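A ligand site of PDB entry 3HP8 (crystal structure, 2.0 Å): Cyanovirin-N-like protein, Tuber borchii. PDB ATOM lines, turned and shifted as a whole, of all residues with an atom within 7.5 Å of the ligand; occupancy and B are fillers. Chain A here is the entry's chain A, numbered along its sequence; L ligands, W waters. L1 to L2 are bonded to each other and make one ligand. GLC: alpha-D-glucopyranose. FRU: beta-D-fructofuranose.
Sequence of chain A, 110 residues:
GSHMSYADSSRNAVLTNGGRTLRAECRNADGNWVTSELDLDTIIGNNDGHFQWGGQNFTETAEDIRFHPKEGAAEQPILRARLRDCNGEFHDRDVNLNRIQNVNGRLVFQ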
ATOM      1  N   ASP A  41     -28.843   0.040 -27.366  1.00  0.00           N
ATOM      2  CA  ASP A  41     -27.942  -1.012 -27.798  1.00  0.00           C
ATOM      3  C   ASP A  41     -27.766  -1.077 -29.329  1.00  0.00           C
ATOM      4  O   ASP A  41     -26.927  -1.836 -29.828  1.00  0.00           O
ATOM      5  CB  ASP A  41     -28.422  -2.346 -27.260  1.00  0.00           C
ATOM      6  CG  ASP A  41     -27.789  -2.691 -25.942  1.00  0.00           C
ATOM      7  OD1 ASP A  41     -26.827  -2.013 -25.551  1.00  0.00           O
ATOM      8  OD2 ASP A  41     -28.236  -3.649 -25.313  1.00  0.00           O
ATOM      9  N   ILE A  44     -24.965   2.492 -29.439  1.00  0.00           N
ATOM     10  CA  ILE A  44     -23.912   2.811 -28.494  1.00  0.00           C
ATOM     11  C   ILE A  44     -23.229   1.496 -28.170  1.00  0.00           C
ATOM     12  O   ILE A  44     -23.887   0.546 -27.783  1.00  0.00           O
ATOM     13  CB  ILE A  44     -24.489   3.433 -27.196  1.00  0.00           C
ATOM     14  CG1 ILE A  44     -25.241   4.735 -27.516  1.00  0.00           C
ATOM     15  CG2 ILE A  44     -23.363   3.684 -26.189  1.00  0.00           C
ATOM     16  CD1 ILE A  44     -25.770   5.483 -26.248  1.00  0.00           C
ATOM     17  N   GLY A  45     -21.920   1.419 -28.410  1.00  0.00           N
ATOM     18  CA  GLY A  45     -21.161   0.229 -28.026  1.00  0.00           C
ATOM     19  C   GLY A  45     -20.245   0.480 -26.866  1.00  0.00           C
ATOM     20  O   GLY A  45     -20.180   1.605 -26.345  1.00  0.00           O
ATOM     21  N   ASN A  46     -19.603  -0.591 -26.407  1.00  0.00           N
ATOM     22  CA  ASN A  46     -18.558  -0.504 -25.427  1.00  0.00           C
ATOM     23  C   ASN A  46     -17.205  -0.789 -26.073  1.00  0.00           C
ATOM     24  O   ASN A  46     -16.922  -1.937 -26.467  1.00  0.00           O
ATOM     25  CB  ASN A  46     -18.795  -1.504 -24.320  1.00  0.00           C
ATOM     26  CG  ASN A  46     -17.617  -1.663 -23.455  1.00  0.00           C
ATOM     27  OD1 ASN A  46     -16.711  -0.824 -23.475  1.00  0.00           O
ATOM     28  ND2 ASN A  46     -17.600  -2.722 -22.651  1.00  0.00           N
ATOM     29  N   ASN A  47     -16.425   0.282 -26.268  1.00  0.00           N
ATOM     30  CA  ASN A  47     -15.117   0.198 -26.926  1.00  0.00           C
ATOM     31  C   ASN A  47     -13.976   0.305 -25.907  1.00  0.00           C
ATOM     32  O   ASN A  47     -13.672   1.383 -25.406  1.00  0.00           O
ATOM     33  CB  ASN A  47     -14.995   1.317 -27.975  1.00  0.00           C
ATOM     34  CG  ASN A  47     -13.761   1.149 -28.859  1.00  0.00           C
ATOM     35  OD1 ASN A  47     -12.907   0.293 -28.636  1.00  0.00           O
ATOM     36  ND2 ASN A  47     -13.687   1.958 -29.881  1.00  0.00           N
ATOM     37  N   ASP A  48     -13.456  -0.846 -25.516  1.00  0.00           N
ATOM     38  CA  ASP A  48     -12.393  -0.982 -24.534  1.00  0.00           C
ATOM     39  C   ASP A  48     -12.773  -0.175 -23.295  1.00  0.00           C
ATOM     40  O   ASP A  48     -11.951   0.548 -22.766  1.00  0.00           O
ATOM     41  CB  ASP A  48     -11.056  -0.491 -25.097  1.00  0.00           C
ATOM     42  CG  ASP A  48      -9.855  -0.843 -24.199  1.00  0.00           C
ATOM     43  OD1 ASP A  48      -9.935  -1.740 -23.339  1.00  0.00           O
ATOM     44  OD2 ASP A  48      -8.825  -0.157 -24.307  1.00  0.00           O
ATOM     45  N   GLY A  49     -14.011  -0.347 -22.817  1.00  0.00           N
ATOM     46  CA  GLY A  49     -14.413   0.268 -21.526  1.00  0.00           C
ATOM     47  C   GLY A  49     -14.837   1.731 -21.648  1.00  0.00           C
ATOM     48  O   GLY A  49     -14.897   2.447 -20.655  1.00  0.00           O
ATOM     49  N   HIS A  50     -15.104   2.147 -22.874  1.00  0.00           N
ATOM     50  CA  HIS A  50     -15.635   3.478 -23.216  1.00  0.00           C
ATOM     51  C   HIS A  50     -16.901   3.397 -24.078  1.00  0.00           C
ATOM     52  O   HIS A  50     -17.017   2.538 -24.956  1.00  0.00           O
ATOM     53  CB  HIS A  50     -14.559   4.265 -23.994  1.00  0.00           C
ATOM     54  CG  HIS A  50     -13.348   4.582 -23.190  1.00  0.00           C
ATOM     55  ND1 HIS A  50     -13.268   5.713 -22.401  1.00  0.00           N
ATOM     56  CD2 HIS A  50     -12.216   3.882 -22.955  1.00  0.00           C
ATOM     57  CE1 HIS A  50     -12.110   5.722 -21.762  1.00  0.00           C
ATOM     58  NE2 HIS A  50     -11.471   4.604 -22.055  1.00  0.00           N
ATOM     59  N   GLN A  52     -19.231   4.191 -27.112  1.00  0.00           N
ATOM     60  CA  GLN A  52     -18.873   4.405 -28.518  1.00  0.00           C
ATOM     61  C   GLN A  52     -20.121   4.624 -29.340  1.00  0.00           C
ATOM     62  O   GLN A  52     -20.917   3.682 -29.530  1.00  0.00           O
ATOM     63  CB  GLN A  52     -18.199   3.156 -29.081  1.00  0.00           C
ATOM     64  CG  GLN A  52     -17.709   3.300 -30.518  1.00  0.00           C
ATOM     65  CD  GLN A  52     -16.655   4.385 -30.639  1.00  0.00           C
ATOM     66  OE1 GLN A  52     -15.576   4.290 -30.048  1.00  0.00           O
ATOM     67  NE2 GLN A  52     -16.974   5.455 -31.374  1.00  0.00           N
ATOM     68  N   GLY A  55     -21.549   2.206 -32.133  1.00  0.00           N
ATOM     69  CA  GLY A  55     -21.334   0.822 -31.657  1.00  0.00           C
ATOM     70  C   GLY A  55     -22.661   0.140 -31.392  1.00  0.00           C
ATOM     71  O   GLY A  55     -23.720   0.658 -31.786  1.00  0.00           O
ATOM     72  N   GLN A  56     -22.610  -1.016 -30.746  1.00  0.00           N
ATOM     73  CA  GLN A  56     -23.821  -1.731 -30.402  1.00  0.00           C
ATOM     74  C   GLN A  56     -23.577  -2.487 -29.108  1.00  0.00           C
ATOM     75  O   GLN A  56     -22.421  -2.703 -28.730  1.00  0.00           O
ATOM     76  CB  GLN A  56     -24.237  -2.705 -31.508  1.00  0.00           C
ATOM     77  CG  GLN A  56     -23.231  -3.825 -31.747  1.00  0.00           C
ATOM     78  CD  GLN A  56     -23.376  -4.447 -33.134  1.00  0.00           C
ATOM     79  OE1 GLN A  56     -24.395  -4.259 -33.818  1.00  0.00           O
ATOM     80  NE2 GLN A  56     -22.344  -5.193 -33.561  1.00  0.00           N
ATOM     81  N   ASN A  57     -24.653  -2.749 -28.386  1.00  0.00           N
ATOM     82  CA  ASN A  57     -24.641  -3.682 -27.268  1.00  0.00           C
ATOM     83  C   ASN A  57     -23.865  -3.237 -26.060  1.00  0.00           C
ATOM     84  O   ASN A  57     -23.381  -4.066 -25.291  1.00  0.00           O
ATOM     85  CB  ASN A  57     -24.121  -5.053 -27.731  1.00  0.00           C
ATOM     86  CG  ASN A  57     -24.992  -5.677 -28.766  1.00  0.00           C
ATOM     87  OD1 ASN A  57     -24.506  -6.281 -29.728  1.00  0.00           O
ATOM     88  ND2 ASN A  57     -26.281  -5.541 -28.597  1.00  0.00           N
ATOM     89  N   PHE A  58     -23.767  -1.935 -25.841  1.00  0.00           N
ATOM     90  CA  PHE A  58     -23.149  -1.441 -24.611  1.00  0.00           C
ATOM     91  C   PHE A  58     -23.669  -2.057 -23.299  1.00  0.00           C
ATOM     92  O   PHE A  58     -22.901  -2.112 -22.307  1.00  0.00           O
ATOM     93  CB  PHE A  58     -23.150   0.092 -24.537  1.00  0.00           C
ATOM     94  CG  PHE A  58     -24.383   0.671 -23.870  1.00  0.00           C
ATOM     95  CD1 PHE A  58     -25.555   0.844 -24.594  1.00  0.00           C
ATOM     96  CD2 PHE A  58     -24.392   0.893 -22.495  1.00  0.00           C
ATOM     97  CE1 PHE A  58     -26.709   1.336 -23.988  1.00  0.00           C
ATOM     98  CE2 PHE A  58     -25.528   1.375 -21.859  1.00  0.00           C
ATOM     99  CZ  PHE A  58     -26.700   1.601 -22.615  1.00  0.00           C
ATOM    100  N   THR A  59     -24.908  -2.553 -23.278  1.00  0.00           N
ATOM    101  CA  THR A  59     -25.505  -3.051 -22.008  1.00  0.00           C
ATOM    102  C   THR A  59     -25.031  -4.444 -21.675  1.00  0.00           C
ATOM    103  O   THR A  59     -25.322  -4.979 -20.591  1.00  0.00           O
ATOM    104  CB  THR A  59     -27.076  -3.107 -21.987  1.00  0.00           C
ATOM    105  OG1 THR A  59     -27.571  -4.033 -22.976  1.00  0.00           O
ATOM    106  CG2 THR A  59     -27.722  -1.703 -22.152  1.00  0.00           C
ATOM    107  N   GLU A  60     -24.434  -5.110 -22.664  1.00  0.00           N
ATOM    108  CA  GLU A  60     -24.173  -6.495 -22.555  1.00  0.00           C
ATOM    109  C   GLU A  60     -23.602  -6.934 -21.201  1.00  0.00           C
ATOM    110  O   GLU A  60     -24.083  -7.914 -20.663  1.00  0.00           O
ATOM    111  CB  GLU A  60     -23.263  -6.962 -23.719  1.00  0.00           C
ATOM    112  CG  GLU A  60     -22.813  -8.374 -23.504  1.00  0.00           C
ATOM    113  CD  GLU A  60     -21.700  -8.798 -24.466  1.00  0.00           C
ATOM    114  OE1 GLU A  60     -22.001  -9.080 -25.636  1.00  0.00           O
ATOM    115  OE2 GLU A  60     -20.523  -8.846 -24.026  1.00  0.00           O
ATOM    116  N   THR A  61     -22.519  -6.302 -20.731  1.00  0.00           N
ATOM    117  CA  THR A  61     -22.001  -6.571 -19.386  1.00  0.00           C
ATOM    118  C   THR A  61     -21.955  -5.334 -18.502  1.00  0.00           C
ATOM    119  O   THR A  61     -21.265  -5.310 -17.479  1.00  0.00           O
ATOM    120  CB  THR A  61     -20.614  -7.271 -19.398  1.00  0.00           C
ATOM    121  OG1 THR A  61     -19.636  -6.457 -20.062  1.00  0.00           O
ATOM    122  CG2 THR A  61     -20.752  -8.665 -20.089  1.00  0.00           C
ATOM    123  N   ALA A  62     -22.597  -4.255 -18.948  1.00  0.00           N
ATOM    124  CA  ALA A  62     -22.459  -2.980 -18.251  1.00  0.00           C
ATOM    125  C   ALA A  62     -23.076  -3.154 -16.863  1.00  0.00           C
ATOM    126  O   ALA A  62     -24.035  -3.901 -16.722  1.00  0.00           O
ATOM    127  CB  ALA A  62     -23.212  -1.877 -19.022  1.00  0.00           C
ATOM    128  N   LEU A  83     -18.299   0.084 -17.362  1.00  0.00           N
ATOM    129  CA  LEU A  83     -18.102  -0.645 -18.621  1.00  0.00           C
ATOM    130  C   LEU A  83     -16.825  -1.491 -18.529  1.00  0.00           C
ATOM    131  O   LEU A  83     -15.803  -1.040 -18.028  1.00  0.00           O
ATOM    132  CB  LEU A  83     -17.966   0.340 -19.779  1.00  0.00           C
ATOM    133  CG  LEU A  83     -19.184   1.187 -20.208  1.00  0.00           C
ATOM    134  CD1 LEU A  83     -18.845   1.970 -21.495  1.00  0.00           C
ATOM    135  CD2 LEU A  83     -20.398   0.253 -20.427  1.00  0.00           C
ATOM    136  N   ARG A  84     -16.905  -2.715 -19.079  1.00  0.00           N
ATOM    137  CA  ARG A  84     -15.798  -3.661 -19.073  1.00  0.00           C
ATOM    138  C   ARG A  84     -14.778  -3.336 -20.146  1.00  0.00           C
ATOM    139  O   ARG A  84     -15.107  -3.293 -21.356  1.00  0.00           O
ATOM    140  CB  ARG A  84     -16.365  -5.035 -19.394  1.00  0.00           C
ATOM    141  CG  ARG A  84     -15.494  -6.170 -18.968  1.00  0.00           C
ATOM    142  CD  ARG A  84     -16.196  -7.474 -19.299  1.00  0.00           C
ATOM    143  NE  ARG A  84     -15.344  -8.591 -18.949  1.00  0.00           N
ATOM    144  CZ  ARG A  84     -14.522  -9.186 -19.796  1.00  0.00           C
ATOM    145  NH1 ARG A  84     -14.451  -8.809 -21.061  1.00  0.00           N
ATOM    146  NH2 ARG A  84     -13.792 -10.208 -19.373  1.00  0.00           N
ATOM    147  N   ASP A  85     -13.513  -3.150 -19.738  1.00  0.00           N
ATOM    148  CA  ASP A  85     -12.475  -2.903 -20.732  1.00  0.00           C
ATOM    149  C   ASP A  85     -11.930  -4.190 -21.339  1.00  0.00           C
ATOM    150  O   ASP A  85     -12.445  -5.272 -21.037  1.00  0.00           O
ATOM    151  CB  ASP A  85     -11.381  -1.943 -20.240  1.00  0.00           C
ATOM    152  CG  ASP A  85     -10.473  -2.555 -19.215  1.00  0.00           C
ATOM    153  OD1 ASP A  85     -10.421  -3.795 -19.148  1.00  0.00           O
ATOM    154  OD2 ASP A  85      -9.738  -1.779 -18.546  1.00  0.00           O
ATOM    155  N   CYS A  86     -11.021  -4.077 -22.318  1.00  0.00           N
ATOM    156  CA  CYS A  86     -10.427  -5.260 -22.950  1.00  0.00           C
ATOM    157  C   CYS A  86      -9.744  -6.226 -21.993  1.00  0.00           C
ATOM    158  O   CYS A  86      -9.556  -7.403 -22.305  1.00  0.00           O
ATOM    159  CB  CYS A  86      -9.415  -4.812 -24.006  1.00  0.00           C
ATOM    160  SG  CYS A  86     -10.283  -4.093 -25.365  1.00  0.00           S
ATOM    161  N   ASN A  87      -9.310  -5.704 -20.844  1.00  0.00           N
ATOM    162  CA  ASN A  87      -8.666  -6.506 -19.820  1.00  0.00           C
ATOM    163  C   ASN A  87      -9.673  -7.054 -18.844  1.00  0.00           C
ATOM    164  O   ASN A  87      -9.308  -7.658 -17.849  1.00  0.00           O
ATOM    165  CB  ASN A  87      -7.667  -5.677 -19.018  1.00  0.00           C
ATOM    166  CG  ASN A  87      -6.509  -5.204 -19.850  1.00  0.00           C
ATOM    167  OD1 ASN A  87      -6.071  -5.904 -20.776  1.00  0.00           O
ATOM    168  ND2 ASN A  87      -6.004  -4.004 -19.543  1.00  0.00           N
ATOM    169  N   GLY A  88     -10.950  -6.774 -19.079  1.00  0.00           N
ATOM    170  CA  GLY A  88     -11.963  -7.286 -18.183  1.00  0.00           C
ATOM    171  C   GLY A  88     -12.117  -6.470 -16.921  1.00  0.00           C
ATOM    172  O   GLY A  88     -12.839  -6.865 -16.030  1.00  0.00           O
ATOM    173  N   GLU A  89     -11.462  -5.309 -16.857  1.00  0.00           N
ATOM    174  CA  GLU A  89     -11.681  -4.355 -15.734  1.00  0.00           C
ATOM    175  C   GLU A  89     -12.793  -3.353 -16.023  1.00  0.00           C
ATOM    176  O   GLU A  89     -12.962  -2.887 -17.144  1.00  0.00           O
ATOM    177  CB  GLU A  89     -10.425  -3.535 -15.465  1.00  0.00           C
ATOM    178  CG  GLU A  89      -9.376  -4.233 -14.628  1.00  0.00           C
ATOM    179  CD  GLU A  89      -8.013  -3.644 -14.887  1.00  0.00           C
ATOM    180  OE1 GLU A  89      -7.862  -2.399 -14.753  1.00  0.00           O
ATOM    181  OE2 GLU A  89      -7.111  -4.408 -15.288  1.00  0.00           O
HETATM  182  C1  GLC L   1     -17.254  -6.196 -27.021  1.00  0.00           C
HETATM  183  C2  GLC L   1     -17.854  -6.105 -28.418  1.00  0.00           C
HETATM  184  C3  GLC L   1     -18.428  -4.703 -28.494  1.00  0.00           C
HETATM  185  C4  GLC L   1     -19.580  -4.579 -27.505  1.00  0.00           C
HETATM  186  C5  GLC L   1     -19.078  -4.832 -26.102  1.00  0.00           C
HETATM  187  C6  GLC L   1     -20.227  -4.929 -25.094  1.00  0.00           C
HETATM  188  O2  GLC L   1     -16.872  -6.280 -29.433  1.00  0.00           O
HETATM  189  O3  GLC L   1     -19.050  -4.452 -29.706  1.00  0.00           O
HETATM  190  O4  GLC L   1     -20.017  -3.260 -27.629  1.00  0.00           O
HETATM  191  O5  GLC L   1     -18.317  -6.015 -26.055  1.00  0.00           O
HETATM  192  O6  GLC L   1     -19.605  -4.981 -23.838  1.00  0.00           O
HETATM  193  C1  FRU L   2     -14.209  -6.346 -27.602  1.00  0.00           C
HETATM  194  C2  FRU L   2     -14.924  -5.681 -26.439  1.00  0.00           C
HETATM  195  C3  FRU L   2     -14.220  -4.447 -25.907  1.00  0.00           C
HETATM  196  C4  FRU L   2     -14.889  -4.304 -24.544  1.00  0.00           C
HETATM  197  C5  FRU L   2     -14.885  -5.758 -24.103  1.00  0.00           C
HETATM  198  C6  FRU L   2     -16.102  -6.078 -23.270  1.00  0.00           C
HETATM  199  O1  FRU L   2     -14.353  -5.467 -28.695  1.00  0.00           O
HETATM  200  O2  FRU L   2     -16.219  -5.233 -26.842  1.00  0.00           O
HETATM  201  O3  FRU L   2     -14.423  -3.326 -26.739  1.00  0.00           O
HETATM  202  O4  FRU L   2     -14.119  -3.477 -23.718  1.00  0.00           O
HETATM  203  O5  FRU L   2     -14.919  -6.549 -25.319  1.00  0.00           O
HETATM  204  O6  FRU L   2     -16.188  -7.474 -23.051  1.00  0.00           O
HETATM  205  O   HOH W   1     -19.871  -2.065 -30.734  1.00  0.00           O
HETATM  206  O   HOH W   2     -11.885  -6.313 -30.442  1.00  0.00           O
HETATM  207  O   HOH W   3     -19.137  -7.410 -22.638  1.00  0.00           O
HETATM  208  O   HOH W   4     -17.288  -4.270 -31.798  1.00  0.00           O
HETATM  209  O   HOH W   5     -21.143  -6.323 -30.220  1.00  0.00           O
HETATM  210  O   HOH W   6     -11.798  -2.752 -28.866  1.00  0.00           O
HETATM  211  O   HOH W   7     -21.119  -4.044 -21.980  1.00  0.00           O
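The backbone carbonyl oxygen of Arg 84 lies within hydrogen-bond range of an oxygen (O4) of FRU L2.
NH1 of Arg 84 is in hydrogen-bond range of O6 of FRU L2, at 3.0 Å.
O4 of GLC L1 lies within hydrogen-bond range of O of Gln 56 (2.7 Å).
The backbone NH of Asn 46 lies within hydrogen-bond range of an oxygen (O4) of GLC L1, at 3.0 Å.
An oxygen (O3) of FRU L2 sits at hydrogen-bond distance from the backbone carbonyl oxygen (O) of Asn 46, 2.9 Å away.
An oxygen (O6) of GLC L1 lies within hydrogen-bond range of the side-chain amide nitrogen of Asn 46 (3.2 Å).
The backbone NH (N) of Asp 48 sits at hydrogen-bond distance from an oxygen (O3) of FRU L2 (2.9 Å).
An oxygen (O4) of FRU L2 is in hydrogen-bond range of the backbone NH (N) of Gly 49 (3.3 Å).
O4 of FRU L2 is in hydrogen-bond range of N of Cys 86 (3.5 Å).
The side-chain amide oxygen (OD1) of Asn 46 is in hydrogen-bond range of the backbone NH (N) of His 50, 3.4 Å away.
The side-chain carboxylate of Asp 48 is in hydrogen-bond range of the backbone NH of Cys 86, at 2.8 Å.
The backbone NH (N) of Asn 57 sits at hydrogen-bond distance from the backbone carbonyl oxygen (O) of Ile 44 (3.4 Å).
The backbone NH of Asn 57 is in hydrogen-bond range of the backbone carbonyl oxygen of Asp 41 (2.8 Å).
The side-chain carboxylate of Asp 85 lies within hydrogen-bond range of the backbone NH of Asn 87, 2.8 Å away.
OD1 of Asp 85 lies within hydrogen-bond range of N of Gly 88, at 3.0 Å.
N of Glu 89 lies within hydrogen-bond range of OD1 of Asp 85 (2.9 Å).
N of Gly 45 is in hydrogen-bond range of O of Gln 52, 2.7 Å away.
Residues that only touch the ligand: Asn 57, Asp 85, Asn 47, Gly 45 and Glu 60.
Of the 24 residues printed, 11 come within 4 Å of the ligand.
Along chain A the residues within 4 Å of the ligand span positions 45 to 86.
Water W7 lies within hydrogen-bond range of an oxygen (O6) of GLC L1 (2.6 Å), the backbone carbonyl oxygen (O) of Phe 58 (2.6 Å), the backbone NH (N) of Thr 61 (2.9 Å) and the backbone NH (N) of Ala 62 (3.4 Å).
Water W1 lies within hydrogen-bond range of O3 of GLC L1 and N of Gln 56.
Water W3 lies within hydrogen-bond range of the side-chain carboxylate of Glu 60 (2.4 Å), an oxygen (O6) of GLC L1 (2.7 Å) and the side-chain hydroxyl of Thr 61 (2.8 Å).
Water W5 bridges an oxygen (O3) of GLC L1 (2.9 Å) and the side-chain amide oxygen of Asn 57 (3.4 Å).
Water W6 lies within hydrogen-bond range of the side-chain amide oxygen of Asn 47 (3.2 Å) and an oxygen (O3) of FRU L2 (3.4 Å).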
